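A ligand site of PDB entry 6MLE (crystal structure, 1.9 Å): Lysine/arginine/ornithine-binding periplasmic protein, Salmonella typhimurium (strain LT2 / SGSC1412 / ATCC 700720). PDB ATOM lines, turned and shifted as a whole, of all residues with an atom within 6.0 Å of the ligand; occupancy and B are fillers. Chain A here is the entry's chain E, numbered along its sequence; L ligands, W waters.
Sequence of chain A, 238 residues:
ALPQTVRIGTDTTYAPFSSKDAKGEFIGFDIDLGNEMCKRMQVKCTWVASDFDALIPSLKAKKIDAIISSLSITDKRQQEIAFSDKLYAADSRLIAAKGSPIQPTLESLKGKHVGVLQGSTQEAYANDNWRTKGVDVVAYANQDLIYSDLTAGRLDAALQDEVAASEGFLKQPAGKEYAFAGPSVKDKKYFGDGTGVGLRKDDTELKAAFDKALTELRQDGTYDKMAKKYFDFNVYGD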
ATOM      1  N   THR A  10      -4.716  26.509  18.161  1.00  0.00           N
ATOM      2  CA  THR A  10      -5.099  25.152  18.538  1.00  0.00           C
ATOM      3  C   THR A  10      -5.615  24.435  17.300  1.00  0.00           C
ATOM      4  O   THR A  10      -6.130  25.075  16.385  1.00  0.00           O
ATOM      5  CB  THR A  10      -6.171  25.147  19.647  1.00  0.00           C
ATOM      6  OG1 THR A  10      -6.338  23.815  20.175  1.00  0.00           O
ATOM      7  CG2 THR A  10      -7.519  25.676  19.137  1.00  0.00           C
ATOM      8  N   ASP A  11      -5.453  23.119  17.267  1.00  0.00           N
ATOM      9  CA  ASP A  11      -5.988  22.299  16.192  1.00  0.00           C
ATOM     10  C   ASP A  11      -7.233  21.617  16.718  1.00  0.00           C
ATOM     11  O   ASP A  11      -7.149  20.735  17.574  1.00  0.00           O
ATOM     12  CB  ASP A  11      -4.948  21.273  15.724  1.00  0.00           C
ATOM     13  CG  ASP A  11      -5.547  20.213  14.824  1.00  0.00           C
ATOM     14  OD1 ASP A  11      -6.409  20.545  13.985  1.00  0.00           O
ATOM     15  OD2 ASP A  11      -5.137  19.038  14.951  1.00  0.00           O
ATOM     16  N   THR A  12      -8.381  22.050  16.224  1.00  0.00           N
ATOM     17  CA  THR A  12      -9.685  21.605  16.715  1.00  0.00           C
ATOM     18  C   THR A  12     -10.164  20.285  16.128  1.00  0.00           C
ATOM     19  O   THR A  12     -11.330  20.169  15.766  1.00  0.00           O
ATOM     20  CB  THR A  12     -10.767  22.664  16.418  1.00  0.00           C
ATOM     21  OG1 THR A  12     -10.791  22.958  15.022  1.00  0.00           O
ATOM     22  CG2 THR A  12     -10.456  23.933  17.160  1.00  0.00           C
ATOM     23  N   THR A  13      -9.287  19.305  16.045  1.00  0.00           N
ATOM     24  CA  THR A  13      -9.676  17.978  15.564  1.00  0.00           C
ATOM     25  C   THR A  13      -9.136  16.906  16.506  1.00  0.00           C
ATOM     26  O   THR A  13      -8.675  15.854  16.069  1.00  0.00           O
ATOM     27  CB  THR A  13      -9.161  17.717  14.134  1.00  0.00           C
ATOM     28  OG1 THR A  13      -7.739  17.624  14.147  1.00  0.00           O
ATOM     29  CG2 THR A  13      -9.573  18.817  13.201  1.00  0.00           C
ATOM     30  N   TYR A  14      -9.207  17.174  17.811  1.00  0.00           N
ATOM     31  CA  TYR A  14      -8.606  16.279  18.792  1.00  0.00           C
ATOM     32  C   TYR A  14      -9.481  16.286  20.061  1.00  0.00           C
ATOM     33  O   TYR A  14      -9.040  16.634  21.152  1.00  0.00           O
ATOM     34  CB  TYR A  14      -7.150  16.724  19.068  1.00  0.00           C
ATOM     35  CG  TYR A  14      -6.117  15.603  19.188  1.00  0.00           C
ATOM     36  CD1 TYR A  14      -5.826  14.789  18.095  1.00  0.00           C
ATOM     37  CD2 TYR A  14      -5.400  15.393  20.370  1.00  0.00           C
ATOM     38  CE1 TYR A  14      -4.897  13.787  18.176  1.00  0.00           C
ATOM     39  CE2 TYR A  14      -4.454  14.386  20.459  1.00  0.00           C
ATOM     40  CZ  TYR A  14      -4.202  13.588  19.364  1.00  0.00           C
ATOM     41  OH  TYR A  14      -3.246  12.587  19.461  1.00  0.00           O
ATOM     42  N   SER A  18      -9.567  19.457  22.149  1.00  0.00           N
ATOM     43  CA  SER A  18      -9.888  20.588  21.291  1.00  0.00           C
ATOM     44  C   SER A  18     -10.667  20.129  20.065  1.00  0.00           C
ATOM     45  O   SER A  18     -10.207  19.286  19.282  1.00  0.00           O
ATOM     46  CB  SER A  18      -8.608  21.331  20.861  1.00  0.00           C
ATOM     47  OG  SER A  18      -8.918  22.426  20.005  1.00  0.00           O
ATOM     48  N   ASP A  30      -8.702  21.575  26.569  1.00  0.00           N
ATOM     49  CA  ASP A  30      -7.684  22.565  26.257  1.00  0.00           C
ATOM     50  C   ASP A  30      -8.284  23.966  26.300  1.00  0.00           C
ATOM     51  O   ASP A  30      -7.667  24.915  26.793  1.00  0.00           O
ATOM     52  CB  ASP A  30      -7.062  22.314  24.876  1.00  0.00           C
ATOM     53  CG  ASP A  30      -5.922  21.291  24.914  1.00  0.00           C
ATOM     54  OD1 ASP A  30      -5.447  20.912  26.012  1.00  0.00           O
ATOM     55  OD2 ASP A  30      -5.475  20.879  23.819  1.00  0.00           O
ATOM     56  N   PHE A  52      -2.481  21.044  12.936  1.00  0.00           N
ATOM     57  CA  PHE A  52      -1.543  20.857  14.028  1.00  0.00           C
ATOM     58  C   PHE A  52      -0.101  21.166  13.623  1.00  0.00           C
ATOM     59  O   PHE A  52       0.662  21.735  14.413  1.00  0.00           O
ATOM     60  CB  PHE A  52      -1.645  19.441  14.554  1.00  0.00           C
ATOM     61  CG  PHE A  52      -0.791  19.196  15.757  1.00  0.00           C
ATOM     62  CD1 PHE A  52      -1.172  19.686  16.997  1.00  0.00           C
ATOM     63  CD2 PHE A  52       0.388  18.479  15.650  1.00  0.00           C
ATOM     64  CE1 PHE A  52      -0.383  19.472  18.106  1.00  0.00           C
ATOM     65  CE2 PHE A  52       1.185  18.244  16.754  1.00  0.00           C
ATOM     66  CZ  PHE A  52       0.795  18.737  17.990  1.00  0.00           C
ATOM     67  N   LEU A  55       1.195  24.889  13.904  1.00  0.00           N
ATOM     68  CA  LEU A  55       1.184  25.616  15.181  1.00  0.00           C
ATOM     69  C   LEU A  55       2.560  26.159  15.593  1.00  0.00           C
ATOM     70  O   LEU A  55       2.719  27.350  15.876  1.00  0.00           O
ATOM     71  CB  LEU A  55       0.614  24.717  16.289  1.00  0.00           C
ATOM     72  CG  LEU A  55      -0.887  24.438  16.138  1.00  0.00           C
ATOM     73  CD1 LEU A  55      -1.328  23.301  17.024  1.00  0.00           C
ATOM     74  CD2 LEU A  55      -1.700  25.712  16.450  1.00  0.00           C
ATOM     75  N   SER A  69      -2.805  22.720  22.568  1.00  0.00           N
ATOM     76  CA  SER A  69      -3.309  21.796  21.560  1.00  0.00           C
ATOM     77  C   SER A  69      -2.743  20.398  21.829  1.00  0.00           C
ATOM     78  O   SER A  69      -2.222  19.729  20.914  1.00  0.00           O
ATOM     79  CB  SER A  69      -2.922  22.297  20.162  1.00  0.00           C
ATOM     80  OG  SER A  69      -3.674  21.650  19.146  1.00  0.00           O
ATOM     81  N   SER A  70      -2.846  19.992  23.094  1.00  0.00           N
ATOM     82  CA  SER A  70      -2.260  18.748  23.566  1.00  0.00           C
ATOM     83  C   SER A  70      -0.797  18.651  23.135  1.00  0.00           C
ATOM     84  O   SER A  70      -0.332  17.583  22.730  1.00  0.00           O
ATOM     85  CB  SER A  70      -3.043  17.542  23.014  1.00  0.00           C
ATOM     86  OG  SER A  70      -4.411  17.562  23.401  1.00  0.00           O
ATOM     87  N   LEU A  71      -0.074  19.768  23.210  1.00  0.00           N
ATOM     88  CA  LEU A  71       1.282  19.803  22.672  1.00  0.00           C
ATOM     89  C   LEU A  71       2.269  19.161  23.632  1.00  0.00           C
ATOM     90  O   LEU A  71       2.604  19.732  24.682  1.00  0.00           O
ATOM     91  CB  LEU A  71       1.697  21.247  22.363  1.00  0.00           C
ATOM     92  CG  LEU A  71       3.020  21.389  21.599  1.00  0.00           C
ATOM     93  CD1 LEU A  71       2.871  20.820  20.197  1.00  0.00           C
ATOM     94  CD2 LEU A  71       3.493  22.853  21.526  1.00  0.00           C
ATOM     95  N   SER A  72       2.700  17.960  23.295  1.00  0.00           N
ATOM     96  CA  SER A  72       3.621  17.211  24.147  1.00  0.00           C
ATOM     97  C   SER A  72       4.941  17.944  24.394  1.00  0.00           C
ATOM     98  O   SER A  72       5.568  18.470  23.478  1.00  0.00           O
ATOM     99  CB  SER A  72       3.904  15.845  23.521  1.00  0.00           C
ATOM    100  OG  SER A  72       2.759  15.015  23.630  1.00  0.00           O
ATOM    101  N   ARG A  77      11.419  19.514  20.971  1.00  0.00           N
ATOM    102  CA  ARG A  77      10.682  20.766  20.825  1.00  0.00           C
ATOM    103  C   ARG A  77      11.265  21.878  21.691  1.00  0.00           C
ATOM    104  O   ARG A  77      11.200  23.061  21.325  1.00  0.00           O
ATOM    105  CB  ARG A  77       9.199  20.555  21.155  1.00  0.00           C
ATOM    106  CG  ARG A  77       8.442  19.933  20.002  1.00  0.00           C
ATOM    107  CD  ARG A  77       7.093  19.400  20.453  1.00  0.00           C
ATOM    108  NE  ARG A  77       6.343  18.830  19.352  1.00  0.00           N
ATOM    109  CZ  ARG A  77       5.214  18.138  19.495  1.00  0.00           C
ATOM    110  NH1 ARG A  77       4.728  17.910  20.707  1.00  0.00           N
ATOM    111  NH2 ARG A  77       4.590  17.661  18.429  1.00  0.00           N
ATOM    112  N   ALA A  90       0.006  12.553  28.674  1.00  0.00           N
ATOM    113  CA  ALA A  90      -0.363  12.039  27.363  1.00  0.00           C
ATOM    114  C   ALA A  90       0.511  10.858  26.967  1.00  0.00           C
ATOM    115  O   ALA A  90       1.711  11.010  26.740  1.00  0.00           O
ATOM    116  CB  ALA A  90      -0.274  13.134  26.318  1.00  0.00           C
ATOM    117  N   LEU A 117      -0.961  11.627  12.712  1.00  0.00           N
ATOM    118  CA  LEU A 117      -1.078  13.070  12.532  1.00  0.00           C
ATOM    119  C   LEU A 117       0.228  13.754  12.078  1.00  0.00           C
ATOM    120  O   LEU A 117       1.277  13.578  12.708  1.00  0.00           O
ATOM    121  CB  LEU A 117      -1.552  13.714  13.841  1.00  0.00           C
ATOM    122  CG  LEU A 117      -1.803  15.229  13.855  1.00  0.00           C
ATOM    123  CD1 LEU A 117      -2.836  15.622  12.819  1.00  0.00           C
ATOM    124  CD2 LEU A 117      -2.254  15.650  15.246  1.00  0.00           C
ATOM    125  N   GLY A 119       3.103  16.192  11.831  1.00  0.00           N
ATOM    126  CA  GLY A 119       3.732  17.077  12.802  1.00  0.00           C
ATOM    127  C   GLY A 119       3.636  16.644  14.253  1.00  0.00           C
ATOM    128  O   GLY A 119       4.083  17.365  15.163  1.00  0.00           O
ATOM    129  N   SER A 120       3.052  15.462  14.480  1.00  0.00           N
ATOM    130  CA  SER A 120       2.902  14.912  15.837  1.00  0.00           C
ATOM    131  C   SER A 120       4.122  14.093  16.279  1.00  0.00           C
ATOM    132  O   SER A 120       4.950  13.681  15.462  1.00  0.00           O
ATOM    133  CB  SER A 120       1.665  14.012  15.925  1.00  0.00           C
ATOM    134  OG  SER A 120       1.835  12.819  15.158  1.00  0.00           O
ATOM    135  N   THR A 121       4.206  13.874  17.582  1.00  0.00           N
ATOM    136  CA  THR A 121       5.238  13.001  18.145  1.00  0.00           C
ATOM    137  C   THR A 121       5.041  11.568  17.634  1.00  0.00           C
ATOM    138  O   THR A 121       6.003  10.810  17.453  1.00  0.00           O
ATOM    139  CB  THR A 121       5.209  12.997  19.668  1.00  0.00           C
ATOM    140  OG1 THR A 121       3.936  12.517  20.110  1.00  0.00           O
ATOM    141  CG2 THR A 121       5.432  14.392  20.224  1.00  0.00           C
ATOM    142  N   GLN A 122       3.781  11.214  17.383  1.00  0.00           N
ATOM    143  CA  GLN A 122       3.431   9.901  16.844  1.00  0.00           C
ATOM    144  C   GLN A 122       3.976   9.720  15.429  1.00  0.00           C
ATOM    145  O   GLN A 122       4.460   8.644  15.080  1.00  0.00           O
ATOM    146  CB  GLN A 122       1.899   9.708  16.863  1.00  0.00           C
ATOM    147  CG  GLN A 122       1.304   9.537  18.250  1.00  0.00           C
ATOM    148  CD  GLN A 122       0.886  10.843  18.886  1.00  0.00           C
ATOM    149  OE1 GLN A 122       0.813  11.873  18.226  1.00  0.00           O
ATOM    150  NE2 GLN A 122       0.602  10.810  20.185  1.00  0.00           N
ATOM    151  N   GLN A 143      -6.589  14.587  12.606  1.00  0.00           N
ATOM    152  CA  GLN A 143      -6.972  13.323  13.221  1.00  0.00           C
ATOM    153  C   GLN A 143      -8.345  12.836  12.788  1.00  0.00           C
ATOM    154  O   GLN A 143      -8.617  11.628  12.803  1.00  0.00           O
ATOM    155  CB  GLN A 143      -6.924  13.432  14.750  1.00  0.00           C
ATOM    156  CG  GLN A 143      -7.130  12.106  15.518  1.00  0.00           C
ATOM    157  CD  GLN A 143      -5.985  11.104  15.337  1.00  0.00           C
ATOM    158  OE1 GLN A 143      -4.810  11.477  15.257  1.00  0.00           O
ATOM    159  NE2 GLN A 143      -6.328   9.816  15.302  1.00  0.00           N
ATOM    160  N   ASP A 161      -2.655  10.170  20.737  1.00  0.00           N
ATOM    161  CA  ASP A 161      -2.701  10.202  22.193  1.00  0.00           C
ATOM    162  C   ASP A 161      -3.802   9.251  22.686  1.00  0.00           C
ATOM    163  O   ASP A 161      -4.898   9.193  22.108  1.00  0.00           O
ATOM    164  CB  ASP A 161      -2.958  11.629  22.714  1.00  0.00           C
ATOM    165  CG  ASP A 161      -1.730  12.542  22.602  1.00  0.00           C
ATOM    166  OD1 ASP A 161      -0.607  12.056  22.362  1.00  0.00           O
ATOM    167  OD2 ASP A 161      -1.910  13.774  22.783  1.00  0.00           O
ATOM    168  N   THR A 195       1.671  17.298  28.334  1.00  0.00           N
ATOM    169  CA  THR A 195       1.484  18.408  27.404  1.00  0.00           C
ATOM    170  C   THR A 195       1.601  19.724  28.137  1.00  0.00           C
ATOM    171  O   THR A 195       1.458  19.760  29.360  1.00  0.00           O
ATOM    172  CB  THR A 195       0.097  18.373  26.704  1.00  0.00           C
ATOM    173  OG1 THR A 195      -0.940  18.681  27.655  1.00  0.00           O
ATOM    174  CG2 THR A 195      -0.179  17.004  26.106  1.00  0.00           C
HETATM  175  N1  LIG L   1       0.583  14.923  21.868  1.00  0.00           N
HETATM  176  C1  LIG L   1       0.846  14.772  20.426  1.00  0.00           C
HETATM  177  C2  LIG L   1       1.851  15.810  19.957  1.00  0.00           C
HETATM  178  O1  LIG L   1       2.138  16.770  20.693  1.00  0.00           O
HETATM  179  C3  LIG L   1      -0.438  14.922  19.608  1.00  0.00           C
HETATM  180  C4  LIG L   1      -1.142  16.261  19.837  1.00  0.00           C
HETATM  181  C5  LIG L   1      -2.160  16.582  18.738  1.00  0.00           C
HETATM  182  N2  LIG L   1      -3.050  17.685  19.115  1.00  0.00           N
HETATM  183  C6  LIG L   1      -4.008  18.196  18.342  1.00  0.00           C
HETATM  184  N3  LIG L   1      -4.182  17.725  17.107  1.00  0.00           N
HETATM  185  N4  LIG L   1      -4.773  19.190  18.798  1.00  0.00           N
HETATM  186  O2  LIG L   1       2.373  15.735  18.847  1.00  0.00           O
HETATM  187  O   HOH W   1      -5.653  19.200  21.593  1.00  0.00           O
HETATM  188  O   HOH W   2      -1.600  12.453  17.425  1.00  0.00           O
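O of Asp 11 is in hydrogen-bond range of N4 of the ligand (3.1 Å). The side-chain carboxylate (OD2) of Asp 11 is in salt-bridge range of a nitrogen (N3) of the ligand, 2.7 Å away. O of Ser 69 lies within hydrogen-bond range of N2 of the ligand (2.8 Å). OG of Ser 69 lies within hydrogen-bond range of N4 of the ligand (2.7 Å). N of Ser 72 lies within hydrogen-bond range of O1 of the ligand (2.9 Å). N1 of the ligand is in hydrogen-bond range of OG of Ser 72, 2.8 Å away. O1 of the ligand is in salt-bridge range of NH1 of Arg 77 (2.8 Å). N1 of the ligand lies within salt-bridge range of OD2 of Asp 161, 2.9 Å away. O2 of the ligand sits at hydrogen-bond distance from N of Thr 121. The backbone carbonyl oxygen of Ser 70 sits at hydrogen-bond distance from a nitrogen (N1) of the ligand (2.9 Å).
The side-chain carboxylate of Asp 11 lies within hydrogen-bond range of the side-chain hydroxyl of Thr 13 (3.1 Å). The backbone carbonyl oxygen (O) of Asp 11 is in hydrogen-bond range of the side-chain hydroxyl (OG) of Ser 18 (3.4 Å). The backbone carbonyl oxygen (O) of Ser 72 sits at hydrogen-bond distance from the guanidinium group (NH1) of Arg 77 (2.9 Å). The guanidinium group (NH2) of Arg 77 lies within hydrogen-bond range of the backbone carbonyl oxygen (O) of Gly 119 (3.3 Å). OD1 of Asp 161 lies within hydrogen-bond range of NE2 of Gln 122. N of Ser 70 is in hydrogen-bond range of OD2 of Asp 30 (2.9 Å). The backbone carbonyl oxygen of Leu 117 lies within hydrogen-bond range of the side-chain hydroxyl of Ser 120, 2.6 Å away. The side-chain hydroxyl (OG) of Ser 120 sits close to the backbone NH (N) of Gln 122, 3.4 Å away.
Residues that only touch the ligand: Ser 120, Phe 52, Leu 117, Tyr 14, Gln 122 and Leu 71. Hydrophobic or aromatic side chains that line the ligand: Tyr 14, Phe 52 and Leu 117. Within 4 Å of the ligand: Asp 11, Tyr 14, Phe 52, Ser 69, Ser 70, Leu 71, Ser 72, Arg 77, Leu 117, Ser 120, Thr 121, Gln 122 and Asp 161. Along chain A the residues within 4 Å of the ligand span positions 11 to 161. The nearest printed residue that does not touch the ligand is Gly 119 (4.4 Å).
Water W1 lies within hydrogen-bond range of the side-chain hydroxyl (OG) of Ser 70 (2.7 Å), the side-chain carboxylate (OD2) of Asp 30 (2.8 Å) and a nitrogen (N4) of the ligand (2.9 Å). Water W2 bridges the side-chain amide oxygen of Gln 122 (2.6 Å) and the side-chain hydroxyl of Tyr 14 (2.6 Å).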
